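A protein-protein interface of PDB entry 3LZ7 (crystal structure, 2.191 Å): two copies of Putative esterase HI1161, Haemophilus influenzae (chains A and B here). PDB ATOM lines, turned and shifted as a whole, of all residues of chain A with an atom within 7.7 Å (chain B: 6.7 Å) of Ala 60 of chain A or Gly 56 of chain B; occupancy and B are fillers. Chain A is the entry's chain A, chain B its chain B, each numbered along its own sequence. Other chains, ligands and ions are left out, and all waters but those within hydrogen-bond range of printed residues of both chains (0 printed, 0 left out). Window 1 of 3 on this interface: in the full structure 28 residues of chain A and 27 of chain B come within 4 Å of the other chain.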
ATOM      1  N   ALA A  20     -14.450  16.665 -18.509  1.00  0.00           N
ATOM      2  CA  ALA A  20     -14.742  17.743 -19.464  1.00  0.00           C
ATOM      3  C   ALA A  20     -16.234  18.090 -19.478  1.00  0.00           C
ATOM      4  O   ALA A  20     -16.600  19.238 -19.686  1.00  0.00           O
ATOM      5  CB  ALA A  20     -14.302  17.351 -20.852  1.00  0.00           C
ATOM      6  N   VAL A  21     -17.084  17.086 -19.266  1.00  0.00           N
ATOM      7  CA  VAL A  21     -18.536  17.281 -19.279  1.00  0.00           C
ATOM      8  C   VAL A  21     -18.994  18.268 -18.192  1.00  0.00           C
ATOM      9  O   VAL A  21     -19.610  19.283 -18.503  1.00  0.00           O
ATOM     10  CB  VAL A  21     -19.283  15.933 -19.136  1.00  0.00           C
ATOM     11  CG1 VAL A  21     -20.804  16.140 -19.195  1.00  0.00           C
ATOM     12  CG2 VAL A  21     -18.816  14.956 -20.233  1.00  0.00           C
ATOM     13  N   LEU A  24     -17.600  21.898 -18.511  1.00  0.00           N
ATOM     14  CA  LEU A  24     -18.211  22.775 -19.497  1.00  0.00           C
ATOM     15  C   LEU A  24     -19.650  23.131 -19.117  1.00  0.00           C
ATOM     16  O   LEU A  24     -20.365  23.761 -19.886  1.00  0.00           O
ATOM     17  CB  LEU A  24     -18.163  22.126 -20.879  1.00  0.00           C
ATOM     18  CG  LEU A  24     -16.788  22.094 -21.559  1.00  0.00           C
ATOM     19  CD1 LEU A  24     -16.782  21.123 -22.756  1.00  0.00           C
ATOM     20  CD2 LEU A  24     -16.345  23.495 -21.989  1.00  0.00           C
ATOM     21  N   ILE A  26     -22.089  21.112 -18.775  1.00  0.00           N
ATOM     22  CA  ILE A  26     -23.048  20.246 -19.451  1.00  0.00           C
ATOM     23  C   ILE A  26     -23.858  19.415 -18.466  1.00  0.00           C
ATOM     24  O   ILE A  26     -23.312  18.819 -17.540  1.00  0.00           O
ATOM     25  CB  ILE A  26     -22.357  19.299 -20.448  1.00  0.00           C
ATOM     26  CG1 ILE A  26     -21.677  20.109 -21.559  1.00  0.00           C
ATOM     27  CG2 ILE A  26     -23.365  18.315 -21.012  1.00  0.00           C
ATOM     28  CD1 ILE A  26     -20.758  19.284 -22.459  1.00  0.00           C
ATOM     29  N   MET A  40     -26.357  22.964 -21.952  1.00  0.00           N
ATOM     30  CA  MET A  40     -25.080  23.604 -21.692  1.00  0.00           C
ATOM     31  C   MET A  40     -25.274  25.115 -21.719  1.00  0.00           C
ATOM     32  O   MET A  40     -25.950  25.631 -22.596  1.00  0.00           O
ATOM     33  CB  MET A  40     -24.076  23.212 -22.762  1.00  0.00           C
ATOM     34  CG  MET A  40     -22.698  23.842 -22.607  1.00  0.00           C
ATOM     35  SD  MET A  40     -21.436  23.078 -23.926  1.00  0.00           S
ATOM     36  CE  MET A  40     -22.272  23.805 -25.568  1.00  0.00           C
ATOM     37  N   HIS A  54     -18.784  29.039 -28.667  1.00  0.00           N
ATOM     38  CA  HIS A  54     -17.689  28.478 -29.452  1.00  0.00           C
ATOM     39  C   HIS A  54     -18.211  27.262 -30.227  1.00  0.00           C
ATOM     40  O   HIS A  54     -18.656  26.281 -29.625  1.00  0.00           O
ATOM     41  CB  HIS A  54     -16.601  28.043 -28.469  1.00  0.00           C
ATOM     42  CG  HIS A  54     -15.305  27.650 -29.111  1.00  0.00           C
ATOM     43  ND1 HIS A  54     -15.184  26.561 -29.947  1.00  0.00           N
ATOM     44  CD2 HIS A  54     -14.063  28.183 -29.003  1.00  0.00           C
ATOM     45  CE1 HIS A  54     -13.924  26.445 -30.332  1.00  0.00           C
ATOM     46  NE2 HIS A  54     -13.224  27.413 -29.769  1.00  0.00           N
ATOM     47  N   GLY A  55     -18.168  27.315 -31.554  1.00  0.00           N
ATOM     48  CA  GLY A  55     -18.690  26.226 -32.366  1.00  0.00           C
ATOM     49  C   GLY A  55     -18.061  24.878 -32.051  1.00  0.00           C
ATOM     50  O   GLY A  55     -18.737  23.846 -32.092  1.00  0.00           O
ATOM     51  N   GLY A  56     -16.767  24.879 -31.738  1.00  0.00           N
ATOM     52  CA  GLY A  56     -16.091  23.642 -31.376  1.00  0.00           C
ATOM     53  C   GLY A  56     -16.641  23.055 -30.090  1.00  0.00           C
ATOM     54  O   GLY A  56     -16.711  21.833 -29.924  1.00  0.00           O
ATOM     55  N   VAL A  57     -17.045  23.921 -29.165  1.00  0.00           N
ATOM     56  CA  VAL A  57     -17.608  23.435 -27.906  1.00  0.00           C
ATOM     57  C   VAL A  57     -19.006  22.863 -28.132  1.00  0.00           C
ATOM     58  O   VAL A  57     -19.424  21.959 -27.420  1.00  0.00           O
ATOM     59  CB  VAL A  57     -17.648  24.537 -26.815  1.00  0.00           C
ATOM     60  CG1 VAL A  57     -18.549  24.109 -25.651  1.00  0.00           C
ATOM     61  CG2 VAL A  57     -16.227  24.863 -26.337  1.00  0.00           C
ATOM     62  N   SER A  58     -19.728  23.384 -29.127  1.00  0.00           N
ATOM     63  CA  SER A  58     -21.009  22.784 -29.517  1.00  0.00           C
ATOM     64  C   SER A  58     -20.819  21.331 -29.916  1.00  0.00           C
ATOM     65  O   SER A  58     -21.613  20.457 -29.561  1.00  0.00           O
ATOM     66  CB  SER A  58     -21.631  23.544 -30.687  1.00  0.00           C
ATOM     67  OG  SER A  58     -21.704  24.920 -30.384  1.00  0.00           O
ATOM     68  N   VAL A  59     -19.757  21.070 -30.663  1.00  0.00           N
ATOM     69  CA  VAL A  59     -19.450  19.696 -31.068  1.00  0.00           C
ATOM     70  C   VAL A  59     -19.088  18.823 -29.875  1.00  0.00           C
ATOM     71  O   VAL A  59     -19.487  17.660 -29.805  1.00  0.00           O
ATOM     72  CB  VAL A  59     -18.356  19.650 -32.140  1.00  0.00           C
ATOM     73  CG1 VAL A  59     -18.089  18.211 -32.551  1.00  0.00           C
ATOM     74  CG2 VAL A  59     -18.802  20.482 -33.345  1.00  0.00           C
ATOM     75  N   ALA A  60     -18.370  19.387 -28.911  1.00  0.00           N
ATOM     76  CA  ALA A  60     -18.135  18.665 -27.657  1.00  0.00           C
ATOM     77  C   ALA A  60     -19.446  18.200 -27.008  1.00  0.00           C
ATOM     78  O   ALA A  60     -19.534  17.080 -26.492  1.00  0.00           O
ATOM     79  CB  ALA A  60     -17.323  19.526 -26.679  1.00  0.00           C
ATOM     80  N   LEU A  61     -20.463  19.065 -27.036  1.00  0.00           N
ATOM     81  CA  LEU A  61     -21.777  18.738 -26.478  1.00  0.00           C
ATOM     82  C   LEU A  61     -22.469  17.605 -27.243  1.00  0.00           C
ATOM     83  O   LEU A  61     -23.077  16.713 -26.642  1.00  0.00           O
ATOM     84  CB  LEU A  61     -22.680  19.981 -26.479  1.00  0.00           C
ATOM     85  CG  LEU A  61     -24.124  19.763 -26.015  1.00  0.00           C
ATOM     86  CD1 LEU A  61     -24.143  19.174 -24.613  1.00  0.00           C
ATOM     87  CD2 LEU A  61     -24.898  21.071 -26.048  1.00  0.00           C
ATOM     88  N   ALA A  62     -22.390  17.665 -28.570  1.00  0.00           N
ATOM     89  CA  ALA A  62     -22.961  16.628 -29.438  1.00  0.00           C
ATOM     90  C   ALA A  62     -22.302  15.277 -29.222  1.00  0.00           C
ATOM     91  O   ALA A  62     -22.975  14.263 -29.107  1.00  0.00           O
ATOM     92  CB  ALA A  62     -22.814  17.032 -30.886  1.00  0.00           C
ATOM     93  N   GLU A  63     -20.975  15.254 -29.183  1.00  0.00           N
ATOM     94  CA  GLU A  63     -20.302  13.983 -29.021  1.00  0.00           C
ATOM     95  C   GLU A  63     -20.624  13.409 -27.649  1.00  0.00           C
ATOM     96  O   GLU A  63     -20.794  12.199 -27.508  1.00  0.00           O
ATOM     97  CB  GLU A  63     -18.786  14.102 -29.231  1.00  0.00           C
ATOM     98  CG  GLU A  63     -18.074  12.799 -28.926  1.00  0.00           C
ATOM     99  CD  GLU A  63     -16.931  12.505 -29.889  1.00  0.00           C
ATOM    100  OE1 GLU A  63     -16.738  13.296 -30.845  1.00  0.00           O
ATOM    101  OE2 GLU A  63     -16.233  11.484 -29.681  1.00  0.00           O
ATOM    102  N   THR A  64     -20.731  14.277 -26.645  1.00  0.00           N
ATOM    103  CA  THR A  64     -21.053  13.824 -25.291  1.00  0.00           C
ATOM    104  C   THR A  64     -22.410  13.124 -25.228  1.00  0.00           C
ATOM    105  O   THR A  64     -22.521  12.029 -24.701  1.00  0.00           O
ATOM    106  CB  THR A  64     -21.079  14.992 -24.268  1.00  0.00           C
ATOM    107  OG1 THR A  64     -19.787  15.608 -24.191  1.00  0.00           O
ATOM    108  CG2 THR A  64     -21.464  14.478 -22.893  1.00  0.00           C
ATOM    109  N   ILE A  65     -23.448  13.762 -25.750  1.00  0.00           N
ATOM    110  CA  ILE A  65     -24.798  13.220 -25.563  1.00  0.00           C
ATOM    111  C   ILE A  65     -25.040  12.024 -26.496  1.00  0.00           C
ATOM    112  O   ILE A  65     -25.775  11.110 -26.159  1.00  0.00           O
ATOM    113  CB  ILE A  65     -25.894  14.331 -25.709  1.00  0.00           C
ATOM    114  CG1 ILE A  65     -27.292  13.818 -25.311  1.00  0.00           C
ATOM    115  CG2 ILE A  65     -25.900  14.899 -27.117  1.00  0.00           C
ATOM    116  CD1 ILE A  65     -27.387  13.310 -23.870  1.00  0.00           C
ATOM    117  N   GLY A  66     -24.399  12.022 -27.661  1.00  0.00           N
ATOM    118  CA  GLY A  66     -24.500  10.895 -28.572  1.00  0.00           C
ATOM    119  C   GLY A  66     -23.798   9.632 -28.081  1.00  0.00           C
ATOM    120  O   GLY A  66     -24.311   8.521 -28.253  1.00  0.00           O
ATOM    121  N   SER A  67     -22.615   9.792 -27.491  1.00  0.00           N
ATOM    122  CA  SER A  67     -21.870   8.650 -26.956  1.00  0.00           C
ATOM    123  C   SER A  67     -22.581   8.059 -25.750  1.00  0.00           C
ATOM    124  O   SER A  67     -22.730   6.840 -25.634  1.00  0.00           O
ATOM    125  CB  SER A  67     -20.444   9.063 -26.568  1.00  0.00           C
ATOM    126  OG  SER A  67     -19.826   9.719 -27.666  1.00  0.00           O
ATOM    127  N   ILE A  85     -17.113  12.355 -36.176  1.00  0.00           N
ATOM    128  CA  ILE A  85     -18.246  13.232 -35.979  1.00  0.00           C
ATOM    129  C   ILE A  85     -18.163  14.303 -37.029  1.00  0.00           C
ATOM    130  O   ILE A  85     -17.072  14.667 -37.476  1.00  0.00           O
ATOM    131  CB  ILE A  85     -18.248  13.838 -34.542  1.00  0.00           C
ATOM    132  CG1 ILE A  85     -19.523  14.655 -34.295  1.00  0.00           C
ATOM    133  CG2 ILE A  85     -17.011  14.682 -34.331  1.00  0.00           C
ATOM    134  CD1 ILE A  85     -19.890  14.824 -32.821  1.00  0.00           C
ATOM    135  N   ILE A 118     -28.804  20.480 -32.073  1.00  0.00           N
ATOM    136  CA  ILE A 118     -28.593  21.390 -30.964  1.00  0.00           C
ATOM    137  C   ILE A 118     -29.428  22.645 -31.171  1.00  0.00           C
ATOM    138  O   ILE A 118     -29.338  23.314 -32.206  1.00  0.00           O
ATOM    139  CB  ILE A 118     -27.099  21.736 -30.794  1.00  0.00           C
ATOM    140  CG1 ILE A 118     -26.279  20.452 -30.604  1.00  0.00           C
ATOM    141  CG2 ILE A 118     -26.907  22.668 -29.597  1.00  0.00           C
ATOM    142  CD1 ILE A 118     -24.776  20.697 -30.443  1.00  0.00           C
ATOM    143  N   GLN B  48     -12.907  12.526 -20.953  1.00  0.00           N
ATOM    144  CA  GLN B  48     -14.131  11.797 -20.650  1.00  0.00           C
ATOM    145  C   GLN B  48     -14.116  11.422 -19.178  1.00  0.00           C
ATOM    146  O   GLN B  48     -13.052  11.363 -18.573  1.00  0.00           O
ATOM    147  CB  GLN B  48     -14.175  10.512 -21.478  1.00  0.00           C
ATOM    148  CG  GLN B  48     -14.103  10.748 -22.957  1.00  0.00           C
ATOM    149  CD  GLN B  48     -15.462  11.049 -23.536  1.00  0.00           C
ATOM    150  OE1 GLN B  48     -15.660  10.980 -24.753  1.00  0.00           O
ATOM    151  NE2 GLN B  48     -16.416  11.373 -22.665  1.00  0.00           N
ATOM    152  N   LEU B  53      -8.802  11.364 -23.328  1.00  0.00           N
ATOM    153  CA  LEU B  53      -9.107  12.644 -23.961  1.00  0.00           C
ATOM    154  C   LEU B  53     -10.469  12.606 -24.639  1.00  0.00           C
ATOM    155  O   LEU B  53     -10.753  11.731 -25.447  1.00  0.00           O
ATOM    156  CB  LEU B  53      -8.035  12.999 -24.981  1.00  0.00           C
ATOM    157  CG  LEU B  53      -8.249  14.318 -25.732  1.00  0.00           C
ATOM    158  CD1 LEU B  53      -8.285  15.510 -24.785  1.00  0.00           C
ATOM    159  CD2 LEU B  53      -7.170  14.489 -26.775  1.00  0.00           C
ATOM    160  N   HIS B  54     -11.318  13.556 -24.282  1.00  0.00           N
ATOM    161  CA  HIS B  54     -12.670  13.612 -24.809  1.00  0.00           C
ATOM    162  C   HIS B  54     -12.558  13.989 -26.290  1.00  0.00           C
ATOM    163  O   HIS B  54     -11.983  15.014 -26.623  1.00  0.00           O
ATOM    164  CB  HIS B  54     -13.447  14.656 -24.012  1.00  0.00           C
ATOM    165  CG  HIS B  54     -14.928  14.659 -24.250  1.00  0.00           C
ATOM    166  ND1 HIS B  54     -15.488  14.943 -25.475  1.00  0.00           N
ATOM    167  CD2 HIS B  54     -15.966  14.481 -23.396  1.00  0.00           C
ATOM    168  CE1 HIS B  54     -16.807  14.913 -25.376  1.00  0.00           C
ATOM    169  NE2 HIS B  54     -17.122  14.646 -24.121  1.00  0.00           N
ATOM    170  N   GLY B  55     -13.090  13.155 -27.179  1.00  0.00           N
ATOM    171  CA  GLY B  55     -12.954  13.402 -28.603  1.00  0.00           C
ATOM    172  C   GLY B  55     -13.691  14.650 -29.028  1.00  0.00           C
ATOM    173  O   GLY B  55     -13.310  15.318 -29.988  1.00  0.00           O
ATOM    174  N   GLY B  56     -14.757  14.981 -28.310  1.00  0.00           N
ATOM    175  CA  GLY B  56     -15.462  16.221 -28.587  1.00  0.00           C
ATOM    176  C   GLY B  56     -14.617  17.453 -28.296  1.00  0.00           C
ATOM    177  O   GLY B  56     -14.749  18.482 -28.969  1.00  0.00           O
ATOM    178  N   VAL B  57     -13.751  17.355 -27.285  1.00  0.00           N
ATOM    179  CA  VAL B  57     -12.887  18.476 -26.891  1.00  0.00           C
ATOM    180  C   VAL B  57     -11.702  18.637 -27.849  1.00  0.00           C
ATOM    181  O   VAL B  57     -11.232  19.753 -28.081  1.00  0.00           O
ATOM    182  CB  VAL B  57     -12.381  18.317 -25.418  1.00  0.00           C
ATOM    183  CG1 VAL B  57     -11.251  19.289 -25.113  1.00  0.00           C
ATOM    184  CG2 VAL B  57     -13.540  18.488 -24.433  1.00  0.00           C
ATOM    185  N   SER B  58     -11.222  17.525 -28.405  1.00  0.00           N
ATOM    186  CA  SER B  58     -10.250  17.583 -29.517  1.00  0.00           C
ATOM    187  C   SER B  58     -10.821  18.382 -30.674  1.00  0.00           C
ATOM    188  O   SER B  58     -10.116  19.168 -31.304  1.00  0.00           O
ATOM    189  CB  SER B  58      -9.914  16.183 -30.049  1.00  0.00           C
ATOM    190  OG  SER B  58      -9.537  15.337 -29.006  1.00  0.00           O
ATOM    191  N   VAL B  59     -12.108  18.181 -30.963  1.00  0.00           N
ATOM    192  CA  VAL B  59     -12.750  18.988 -31.996  1.00  0.00           C
ATOM    193  C   VAL B  59     -12.793  20.471 -31.614  1.00  0.00           C
ATOM    194  O   VAL B  59     -12.608  21.349 -32.464  1.00  0.00           O
ATOM    195  CB  VAL B  59     -14.170  18.471 -32.329  1.00  0.00           C
ATOM    196  CG1 VAL B  59     -14.799  19.322 -33.419  1.00  0.00           C
ATOM    197  CG2 VAL B  59     -14.088  17.021 -32.752  1.00  0.00           C
ATOM    198  N   ALA B  60     -13.018  20.758 -30.335  1.00  0.00           N
ATOM    199  CA  ALA B  60     -13.002  22.144 -29.895  1.00  0.00           C
ATOM    200  C   ALA B  60     -11.616  22.750 -30.123  1.00  0.00           C
ATOM    201  O   ALA B  60     -11.483  23.903 -30.543  1.00  0.00           O
ATOM    202  CB  ALA B  60     -13.414  22.252 -28.441  1.00  0.00           C
ATOM    203  N   LEU B  61     -10.583  21.960 -29.855  1.00  0.00           N
ATOM    204  CA  LEU B  61      -9.208  22.391 -30.098  1.00  0.00           C
ATOM    205  C   LEU B  61      -9.010  22.645 -31.575  1.00  0.00           C
ATOM    206  O   LEU B  61      -8.427  23.654 -31.960  1.00  0.00           O
ATOM    207  CB  LEU B  61      -8.201  21.343 -29.597  1.00  0.00           C
ATOM    208  CG  LEU B  61      -6.720  21.578 -29.913  1.00  0.00           C
ATOM    209  CD1 LEU B  61      -6.272  22.980 -29.508  1.00  0.00           C
ATOM    210  CD2 LEU B  61      -5.842  20.511 -29.230  1.00  0.00           C
ATOM    211  N   HIS B  89     -11.445  10.305 -34.846  1.00  0.00           N
ATOM    212  CA  HIS B  89     -10.607  10.040 -33.687  1.00  0.00           C
ATOM    213  C   HIS B  89      -9.853   8.733 -33.928  1.00  0.00           C
ATOM    214  O   HIS B  89     -10.461   7.697 -34.168  1.00  0.00           O
ATOM    215  CB  HIS B  89     -11.462  10.020 -32.413  1.00  0.00           C
ATOM    216  CG  HIS B  89     -12.299  11.252 -32.262  1.00  0.00           C
ATOM    217  ND1 HIS B  89     -13.676  11.239 -32.352  1.00  0.00           N
ATOM    218  CD2 HIS B  89     -11.947  12.548 -32.112  1.00  0.00           C
ATOM    219  CE1 HIS B  89     -14.137  12.469 -32.239  1.00  0.00           C
ATOM    220  NE2 HIS B  89     -13.109  13.284 -32.093  1.00  0.00           N
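A ring nitrogen (NE2) of His 54 of chain B lies within hydrogen-bond range of the side-chain hydroxyl (OG1) of Thr 64 of chain A (2.8 Å).
ND1 of His 54 of chain A lies within hydrogen-bond range of N of Gly 56 of chain A (2.9 Å). O of Gly 55 of chain B sits at hydrogen-bond distance from NE2 of His 89 of chain B (2.9 Å). The backbone carbonyl oxygen (O) of His 54 of chain B sits at hydrogen-bond distance from the side-chain hydroxyl (OG) of Ser 58 of chain B. O of Glu 63 of chain A sits at hydrogen-bond distance from OG of Ser 67 of chain A (2.7 Å). ND1 of His 54 of chain A sits at hydrogen-bond distance from N of Val 57 of chain A, at 3.3 Å. The backbone carbonyl oxygen (O) of Ala 60 of chain A lies within hydrogen-bond range of the side-chain hydroxyl (OG1) of Thr 64 of chain A (2.7 Å).
Among the printed residues, merely in contact across the chains: Ala 20 of chain A with Val 57 of chain B, His 54 of chain A with Ala 60 of chain B, Gly 56 of chain A with Gly 56 of chain B, Gly 56 of chain A with Ala 60 of chain B, Val 59 of chain A with Val 59 of chain B, Ala 60 of chain A with His 54 of chain B, Ala 60 of chain A with Gly 56 of chain B, Glu 63 of chain A with Gly 55 of chain B, Glu 63 of chain A with Gly 56 of chain B and Glu 63 of chain A with His 89 of chain B.
Of the printed residues of chain B, Val 59 of chain A touches Val 59. Ile 118 of chain A touches none of the printed residues of chain B. Gly 55 of chain B touches one residue of chain A. Of the printed residues of chain A, Gly 56 of chain B touches Gly 56, Ala 60 and Glu 63. Printed residues of chain A within 4 Å of Val 57 of chain B: Ala 20 (3.8 Å). Printed residues of chain A within 4 Å of Val 59 of chain B: Val 59. Printed residues of chain A within 4 Å of Ala 60 of chain B: His 54 and Gly 56. Of the printed residues of chain A, His 89 of chain B touches Glu 63. The nearest residue of chain B that does not touch Ala 60 of chain A is Val 57 of chain B (4.2 Å).
Hydrophobic or aromatic side chains of chain A that line the printed part of chain B: Ala 20, His 54, Val 59 and Ala 60. Printed residues of chain B that touch a printed residue of chain A: His 54, Gly 55, Gly 56, Val 57, Val 59, Ala 60 and His 89. Hydrophobic or aromatic side chains of chain B within 4 Å of the printed part of chain A: His 54, Val 57, Val 59, Ala 60 and His 89. Among the printed residues, 11 pairs touch across the chains.
His 54 of chain A touches Ala 60 of chain B, and with the chains exchanged Ala 60 of chain A touches His 54 of chain B. Gly 56 of chain A touches its own counterpart, Gly 56 of chain B. Gly 56 of chain A touches Ala 60 of chain B, and with the chains exchanged Ala 60 of chain A touches Gly 56 of chain B. Val 59 of chain A touches its own counterpart, Val 59 of chain B. 8 positions are printed for both chains. Of the 11 pairs that touch across the chains among the printed residues, 6 have their exchanged pair printed and touching as well.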
